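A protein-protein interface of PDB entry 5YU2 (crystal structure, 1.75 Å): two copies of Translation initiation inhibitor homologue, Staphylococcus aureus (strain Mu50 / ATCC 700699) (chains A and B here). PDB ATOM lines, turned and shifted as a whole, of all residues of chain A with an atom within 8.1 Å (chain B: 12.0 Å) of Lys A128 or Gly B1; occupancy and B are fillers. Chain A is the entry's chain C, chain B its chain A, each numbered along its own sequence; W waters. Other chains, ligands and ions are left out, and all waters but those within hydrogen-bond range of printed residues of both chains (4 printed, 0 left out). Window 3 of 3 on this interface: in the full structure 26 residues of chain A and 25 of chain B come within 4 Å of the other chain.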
ATOM      1  N   GLY A  28     -18.938 -10.519  15.707  1.00  0.00           N
ATOM      2  CA  GLY A  28     -17.700 -10.682  14.933  1.00  0.00           C
ATOM      3  C   GLY A  28     -16.513 -11.227  15.726  1.00  0.00           C
ATOM      4  O   GLY A  28     -15.369 -11.261  15.207  1.00  0.00           O
ATOM      5  N   MET A  29     -16.794 -11.654  16.948  1.00  0.00           N
ATOM      6  CA  MET A  29     -15.762 -12.202  17.851  1.00  0.00           C
ATOM      7  C   MET A  29     -16.079 -13.647  18.229  1.00  0.00           C
ATOM      8  O   MET A  29     -17.241 -14.072  18.365  1.00  0.00           O
ATOM      9  CB  MET A  29     -15.581 -11.355  19.105  1.00  0.00           C
ATOM     10  CG  MET A  29     -15.295  -9.849  18.842  1.00  0.00           C
ATOM     11  SD  MET A  29     -13.721  -9.587  18.049  1.00  0.00           S
ATOM     12  CE  MET A  29     -12.613 -10.050  19.415  1.00  0.00           C
ATOM     13  N   VAL A  30     -15.010 -14.460  18.387  1.00  0.00           N
ATOM     14  CA  VAL A  30     -15.129 -15.802  18.821  1.00  0.00           C
ATOM     15  C   VAL A  30     -14.659 -15.892  20.269  1.00  0.00           C
ATOM     16  O   VAL A  30     -13.631 -15.352  20.615  1.00  0.00           O
ATOM     17  CB  VAL A  30     -14.171 -16.736  18.016  1.00  0.00           C
ATOM     18  CG1 VAL A  30     -14.423 -18.180  18.355  1.00  0.00           C
ATOM     19  CG2 VAL A  30     -14.398 -16.476  16.544  1.00  0.00           C
ATOM     20  N   LEU A  64     -10.863 -22.287  16.319  1.00  0.00           N
ATOM     21  CA  LEU A  64     -10.773 -21.006  15.632  1.00  0.00           C
ATOM     22  C   LEU A  64     -11.062 -21.173  14.161  1.00  0.00           C
ATOM     23  O   LEU A  64     -11.863 -20.415  13.608  1.00  0.00           O
ATOM     24  CB  LEU A  64      -9.414 -20.353  15.811  1.00  0.00           C
ATOM     25  CG  LEU A  64      -9.142 -19.887  17.243  1.00  0.00           C
ATOM     26  CD1 LEU A  64      -7.735 -19.307  17.244  1.00  0.00           C
ATOM     27  CD2 LEU A  64     -10.178 -18.885  17.724  1.00  0.00           C
ATOM     28  N   GLU A  65     -10.517 -22.213  13.556  1.00  0.00           N
ATOM     29  CA  GLU A  65     -10.711 -22.332  12.114  1.00  0.00           C
ATOM     30  C   GLU A  65     -12.188 -22.675  11.746  1.00  0.00           C
ATOM     31  O   GLU A  65     -12.715 -22.063  10.777  1.00  0.00           O
ATOM     32  CB  GLU A  65      -9.644 -23.232  11.528  1.00  0.00           C
ATOM     33  CG  GLU A  65      -8.317 -22.436  11.514  1.00  0.00           C
ATOM     34  CD  GLU A  65      -7.086 -23.244  11.108  1.00  0.00           C
ATOM     35  OE1 GLU A  65      -7.250 -24.387  10.688  1.00  0.00           O
ATOM     36  OE2 GLU A  65      -5.935 -22.738  11.207  1.00  0.00           O
ATOM     37  N   ALA A  67     -14.757 -21.690  13.415  1.00  0.00           N
ATOM     38  CA  ALA A  67     -15.479 -20.452  13.609  1.00  0.00           C
ATOM     39  C   ALA A  67     -15.245 -19.415  12.543  1.00  0.00           C
ATOM     40  O   ALA A  67     -15.927 -18.405  12.577  1.00  0.00           O
ATOM     41  CB  ALA A  67     -15.121 -19.844  14.943  1.00  0.00           C
ATOM     42  N   GLY A  68     -14.271 -19.596  11.674  1.00  0.00           N
ATOM     43  CA  GLY A  68     -13.877 -18.620  10.674  1.00  0.00           C
ATOM     44  C   GLY A  68     -12.862 -17.597  11.164  1.00  0.00           C
ATOM     45  O   GLY A  68     -12.772 -16.497  10.613  1.00  0.00           O
ATOM     46  N   SER A  69     -12.052 -18.002  12.149  1.00  0.00           N
ATOM     47  CA  SER A  69     -10.964 -17.168  12.647  1.00  0.00           C
ATOM     48  C   SER A  69      -9.690 -17.967  12.481  1.00  0.00           C
ATOM     49  O   SER A  69      -9.620 -18.918  11.686  1.00  0.00           O
ATOM     50  CB  SER A  69     -11.246 -16.714  14.071  1.00  0.00           C
ATOM     51  OG  SER A  69     -10.250 -15.835  14.593  1.00  0.00           O
ATOM     52  N   ASP A  70      -8.646 -17.536  13.132  1.00  0.00           N
ATOM     53  CA  ASP A  70      -7.378 -18.237  13.097  1.00  0.00           C
ATOM     54  C   ASP A  70      -6.469 -17.717  14.213  1.00  0.00           C
ATOM     55  O   ASP A  70      -6.777 -16.766  14.840  1.00  0.00           O
ATOM     56  CB  ASP A  70      -6.706 -18.196  11.727  1.00  0.00           C
ATOM     57  CG  ASP A  70      -6.240 -16.806  11.297  1.00  0.00           C
ATOM     58  OD1 ASP A  70      -6.167 -15.870  12.111  1.00  0.00           O
ATOM     59  OD2 ASP A  70      -5.943 -16.716  10.093  1.00  0.00           O
ATOM     60  N   LEU A  71      -5.360 -18.394  14.459  1.00  0.00           N
ATOM     61  CA  LEU A  71      -4.481 -17.909  15.534  1.00  0.00           C
ATOM     62  C   LEU A  71      -3.891 -16.516  15.343  1.00  0.00           C
ATOM     63  O   LEU A  71      -3.601 -15.831  16.292  1.00  0.00           O
ATOM     64  CB  LEU A  71      -3.317 -18.908  15.734  1.00  0.00           C
ATOM     65  CG  LEU A  71      -3.740 -20.259  16.254  1.00  0.00           C
ATOM     66  CD1 LEU A  71      -2.632 -21.275  16.080  1.00  0.00           C
ATOM     67  CD2 LEU A  71      -4.183 -20.171  17.672  1.00  0.00           C
ATOM     68  N   ASN A  72      -3.741 -16.067  14.106  1.00  0.00           N
ATOM     69  CA  ASN A  72      -3.252 -14.747  13.834  1.00  0.00           C
ATOM     70  C   ASN A  72      -4.279 -13.647  14.103  1.00  0.00           C
ATOM     71  O   ASN A  72      -3.962 -12.472  13.898  1.00  0.00           O
ATOM     72  CB  ASN A  72      -2.779 -14.695  12.394  1.00  0.00           C
ATOM     73  CG  ASN A  72      -1.439 -15.385  12.210  1.00  0.00           C
ATOM     74  OD1 ASN A  72      -0.721 -15.675  13.165  1.00  0.00           O
ATOM     75  ND2 ASN A  72      -1.101 -15.670  10.947  1.00  0.00           N
ATOM     76  N   SER A  73      -5.502 -14.047  14.417  1.00  0.00           N
ATOM     77  CA  SER A  73      -6.612 -13.147  14.639  1.00  0.00           C
ATOM     78  C   SER A  73      -6.993 -13.057  16.130  1.00  0.00           C
ATOM     79  O   SER A  73      -8.033 -12.413  16.495  1.00  0.00           O
ATOM     80  CB  SER A  73      -7.801 -13.523  13.772  1.00  0.00           C
ATOM     81  OG  SER A  73      -7.435 -13.432  12.396  1.00  0.00           O
ATOM     82  N   SER A 125     -11.080 -14.149  19.913  1.00  0.00           N
ATOM     83  CA  SER A 125     -10.442 -13.876  18.584  1.00  0.00           C
ATOM     84  C   SER A 125     -11.444 -13.223  17.654  1.00  0.00           C
ATOM     85  O   SER A 125     -12.641 -13.316  17.875  1.00  0.00           O
ATOM     86  CB  SER A 125     -10.051 -15.200  17.972  1.00  0.00           C
ATOM     87  OG  SER A 125      -9.049 -15.110  16.991  1.00  0.00           O
ATOM     88  N   LYS A 126     -10.939 -12.602  16.622  1.00  0.00           N
ATOM     89  CA  LYS A 126     -11.838 -11.906  15.635  1.00  0.00           C
ATOM     90  C   LYS A 126     -12.056 -12.777  14.410  1.00  0.00           C
ATOM     91  O   LYS A 126     -11.122 -13.389  13.901  1.00  0.00           O
ATOM     92  CB  LYS A 126     -11.232 -10.542  15.319  1.00  0.00           C
ATOM     93  CG  LYS A 126     -12.085  -9.698  14.340  1.00  0.00           C
ATOM     94  CD  LYS A 126     -11.526  -8.292  14.122  1.00  0.00           C
ATOM     95  CE  LYS A 126     -12.243  -7.652  12.890  1.00  0.00           C
ATOM     96  NZ  LYS A 126     -11.704  -6.283  12.797  1.00  0.00           N
ATOM     97  N   ILE A 127     -13.290 -12.748  13.892  1.00  0.00           N
ATOM     98  CA  ILE A 127     -13.660 -13.400  12.637  1.00  0.00           C
ATOM     99  C   ILE A 127     -13.015 -12.721  11.481  1.00  0.00           C
ATOM    100  O   ILE A 127     -12.939 -11.467  11.470  1.00  0.00           O
ATOM    101  CB  ILE A 127     -15.181 -13.395  12.469  1.00  0.00           C
ATOM    102  CG1 ILE A 127     -15.874 -14.175  13.568  1.00  0.00           C
ATOM    103  CG2 ILE A 127     -15.577 -13.994  11.106  1.00  0.00           C
ATOM    104  CD1 ILE A 127     -15.407 -15.592  13.670  1.00  0.00           C
ATOM    105  N   LYS A 128     -12.483 -13.507  10.557  1.00  0.00           N
ATOM    106  CA  LYS A 128     -11.885 -13.002   9.339  1.00  0.00           C
ATOM    107  C   LYS A 128     -12.888 -12.688   8.299  1.00  0.00           C
ATOM    108  O   LYS A 128     -13.775 -13.482   8.054  1.00  0.00           O
ATOM    109  CB  LYS A 128     -10.951 -14.000   8.760  1.00  0.00           C
ATOM    110  CG  LYS A 128      -9.779 -14.206   9.683  1.00  0.00           C
ATOM    111  CD  LYS A 128      -8.666 -14.989   8.991  1.00  0.00           C
ATOM    112  CE  LYS A 128      -9.092 -16.384   8.642  1.00  0.00           C
ATOM    113  NZ  LYS A 128      -7.919 -17.092   8.064  1.00  0.00           N
ATOM    114  N   GLU A 129     -12.731 -11.473   7.776  1.00  0.00           N
ATOM    115  CA  GLU A 129     -13.449 -10.799   6.661  1.00  0.00           C
ATOM    116  C   GLU A 129     -14.965 -10.928   6.617  1.00  0.00           C
ATOM    117  O   GLU A 129     -15.511 -11.638   5.763  1.00  0.00           O
ATOM    118  CB  GLU A 129     -12.728 -10.968   5.285  1.00  0.00           C
ATOM    119  CG  GLU A 129     -12.674 -12.364   4.688  1.00  0.00           C
ATOM    120  CD  GLU A 129     -13.631 -12.588   3.515  1.00  0.00           C
ATOM    121  OE1 GLU A 129     -13.790 -13.765   3.103  1.00  0.00           O
ATOM    122  OE2 GLU A 129     -14.225 -11.614   2.995  1.00  0.00           O
ATOM    123  N   LEU A 130     -15.623 -10.208   7.544  1.00  0.00           N
ATOM    124  CA  LEU A 130     -17.091  -9.953   7.528  1.00  0.00           C
ATOM    125  C   LEU A 130     -17.401  -8.626   8.204  1.00  0.00           C
ATOM    126  O   LEU A 130     -16.552  -8.022   8.881  1.00  0.00           O
ATOM    127  CB  LEU A 130     -17.921 -11.083   8.202  1.00  0.00           C
ATOM    128  CG  LEU A 130     -18.606 -12.165   7.320  1.00  0.00           C
ATOM    129  CD1 LEU A 130     -18.010 -13.562   7.547  1.00  0.00           C
ATOM    130  CD2 LEU A 130     -20.120 -12.204   7.544  1.00  0.00           C
ATOM    131  N   GLY B   1      -4.526 -11.673   5.138  1.00  0.00           N
ATOM    132  CA  GLY B   1      -5.761 -12.403   5.530  1.00  0.00           C
ATOM    133  C   GLY B   1      -6.208 -12.143   6.966  1.00  0.00           C
ATOM    134  O   GLY B   1      -7.418 -12.157   7.212  1.00  0.00           O
ATOM    135  N   ALA B   2      -5.267 -11.887   7.905  1.00  0.00           N
ATOM    136  CA  ALA B   2      -5.639 -11.882   9.351  1.00  0.00           C
ATOM    137  C   ALA B   2      -6.622 -10.787   9.675  1.00  0.00           C
ATOM    138  O   ALA B   2      -6.563  -9.707   9.106  1.00  0.00           O
ATOM    139  CB  ALA B   2      -4.446 -11.782  10.267  1.00  0.00           C
ATOM    140  N   ALA B   3      -7.542 -11.058  10.601  1.00  0.00           N
ATOM    141  CA  ALA B   3      -8.478 -10.010  11.024  1.00  0.00           C
ATOM    142  C   ALA B   3      -7.806  -8.704  11.536  1.00  0.00           C
ATOM    143  O   ALA B   3      -6.775  -8.726  12.245  1.00  0.00           O
ATOM    144  CB  ALA B   3      -9.418 -10.570  12.059  1.00  0.00           C
ATOM    145  N   SER B   4      -8.394  -7.548  11.209  1.00  0.00           N
ATOM    146  CA  SER B   4      -7.675  -6.304  11.450  1.00  0.00           C
ATOM    147  C   SER B   4      -7.824  -5.903  12.950  1.00  0.00           C
ATOM    148  O   SER B   4      -8.923  -6.016  13.592  1.00  0.00           O
ATOM    149  CB  SER B   4      -8.218  -5.224  10.522  1.00  0.00           C
ATOM    150  OG  SER B   4      -9.566  -4.965  10.904  1.00  0.00           O
ATOM    151  N   MET B   5      -6.737  -5.419  13.499  1.00  0.00           N
ATOM    152  CA  MET B   5      -6.668  -5.001  14.895  1.00  0.00           C
ATOM    153  C   MET B   5      -5.404  -4.170  15.039  1.00  0.00           C
ATOM    154  O   MET B   5      -4.563  -4.111  14.097  1.00  0.00           O
ATOM    155  CB  MET B   5      -6.621  -6.248  15.824  1.00  0.00           C
ATOM    156  CG  MET B   5      -5.316  -7.080  15.810  1.00  0.00           C
ATOM    157  SD  MET B   5      -5.429  -8.406  17.070  1.00  0.00           S
ATOM    158  CE  MET B   5      -6.687  -9.416  16.383  1.00  0.00           C
ATOM    159  N   VAL B  26      -9.300  -4.403  19.329  1.00  0.00           N
ATOM    160  CA  VAL B  26     -10.056  -5.224  18.393  1.00  0.00           C
ATOM    161  C   VAL B  26     -11.522  -4.828  18.452  1.00  0.00           C
ATOM    162  O   VAL B  26     -12.140  -4.866  19.507  1.00  0.00           O
ATOM    163  CB  VAL B  26      -9.919  -6.740  18.705  1.00  0.00           C
ATOM    164  CG1 VAL B  26     -10.394  -7.605  17.535  1.00  0.00           C
ATOM    165  CG2 VAL B  26      -8.482  -7.033  19.032  1.00  0.00           C
ATOM    166  N   ASN B  27     -12.056  -4.339  17.322  1.00  0.00           N
ATOM    167  CA  ASN B  27     -13.468  -4.030  17.238  1.00  0.00           C
ATOM    168  C   ASN B  27     -13.910  -3.120  18.361  1.00  0.00           C
ATOM    169  O   ASN B  27     -14.900  -3.369  19.035  1.00  0.00           O
ATOM    170  CB  ASN B  27     -14.333  -5.280  17.157  1.00  0.00           C
ATOM    171  CG  ASN B  27     -14.284  -5.948  15.802  1.00  0.00           C
ATOM    172  OD1 ASN B  27     -13.473  -5.595  14.939  1.00  0.00           O
ATOM    173  ND2 ASN B  27     -15.239  -6.873  15.562  1.00  0.00           N
HETATM  174  O   HOH W   1      -4.274 -14.992   9.018  1.00  0.00           O
HETATM  175  O   HOH W   2     -13.911  -6.875  20.697  1.00  0.00           O
HETATM  176  O   HOH W   3      -4.624  -9.652  13.401  1.00  0.00           O
HETATM  177  O   HOH W   4     -10.402  -4.266  14.963  1.00  0.00           O
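O of Gly A68 sits at hydrogen-bond distance from N of Lys A128 (3.0 Å). OG of Ser A73 is in hydrogen-bond range of OD1 of Asp A70 (2.8 Å). OG of Ser A125 sits at hydrogen-bond distance from O of Ser A73 (2.9 Å). N of Ile A127 sits at hydrogen-bond distance from O of Gly A28 (2.9 Å). The side-chain carboxylate of Asp A70 is in salt-bridge range of the side-chain amino group of Lys A128 (2.9 Å). The backbone carbonyl oxygen (O) of Lys A126 is in hydrogen-bond range of the side-chain hydroxyl (OG) of Ser A69 (2.7 Å).
Water W3 bridges the backbone carbonyl oxygen of Ala B3 (2.6 Å) and the backbone carbonyl oxygen of Asn A72 (2.9 Å). Water W1 lies within hydrogen-bond range of OD2 of Asp A70 (2.6 Å) and N of Ala B2 (3.4 Å). Water W4 lies within hydrogen-bond range of the backbone carbonyl oxygen of Ser B4, the backbone NH of Asn B27 and the side-chain amino group of Lys A126. Water W2 lies within hydrogen-bond range of the backbone carbonyl oxygen (O) of Val B26 and the side-chain sulfur (SD) of Met A29.
The side-chain amino group of Lys A126 lies within hydrogen-bond range of the backbone carbonyl oxygen of Ser B4 (2.9 Å). N of Ala B3 sits at hydrogen-bond distance from OG of Ser A73 (3.0 Å). OD1 of Asn B27 is in hydrogen-bond range of NZ of Lys A126, 2.9 Å away.
CG1 of Val B26 touches CE of Met A29, at 3.8 Å. ND2 of Asn B27 touches SD of Met A29, at 3.98 Å. Ala B2 touches Asn A72. OG of Ser A73 touches CA of Ala B2, at 3.9 Å. Met B5 touches Ser A73 (CE to O, 3.3 Å). CG of Lys A126 touches CB of Ala B3 (3.6 Å). CD of Lys A126 touches CG1 of Val B26 (3.7 Å). Ile A127 touches Ala B3 (O to CB, 3.7 Å). Lys A128 touches Gly B1. Lys A128 touches Ala B3 (CG to N, 3.97 Å).
Lys A128 touches just these residues of chain B: Gly B1 (3.6 Å) and Ala B3 (3.97 Å). Gly B1 touches just one residue of chain A: Lys A128 (3.6 Å). No residue of chain B comes within 4 Å of Ser A69. Printed residues of chain B within 4 Å of Ser A73: Ala B2, Ala B3 and Met B5. Of chain B, only Ala B3 (3.6 Å), Ser B4 (2.9 Å), Val B26 (3.7 Å) and Asn B27 (2.9 Å) come within 4 Å of Lys A126. No residue of chain B comes within 4 Å of Leu A130. Ala B2 touches two residues of chain A. Of the printed residues of chain A, Met B5 touches Ser A73 (3.3 Å). Of the printed residues of chain B, Met A29 touches Val B26 and Asn B27. Printed residues of chain B within 4 Å of Asn A72: Ala B2 (3.7 Å). Of the printed residues of chain A, Ser B4 touches Lys A126. Ser A125 touches none of the printed residues of chain B. Ala A67 touches none of the printed residues of chain B. The nearest residue of chain B that does not touch Lys A128 is Ala B2 (4.4 Å). The nearest printed residue of chain A that does not touch Met B5 is Asn A72 (4.8 Å).
Of the 18 printed residues of chain A, 6 touch a printed residue of chain B. Printed residues of chain B that touch a printed residue of chain A: Gly B1, Ala B2, Ala B3, Ser B4, Met B5, Val B26 and Asn B27. Among the printed residues, no Asp or Glu carboxylate lies within 4 Å of a Lys or Arg side-chain nitrogen of the other chain.
No position is printed for both chains.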
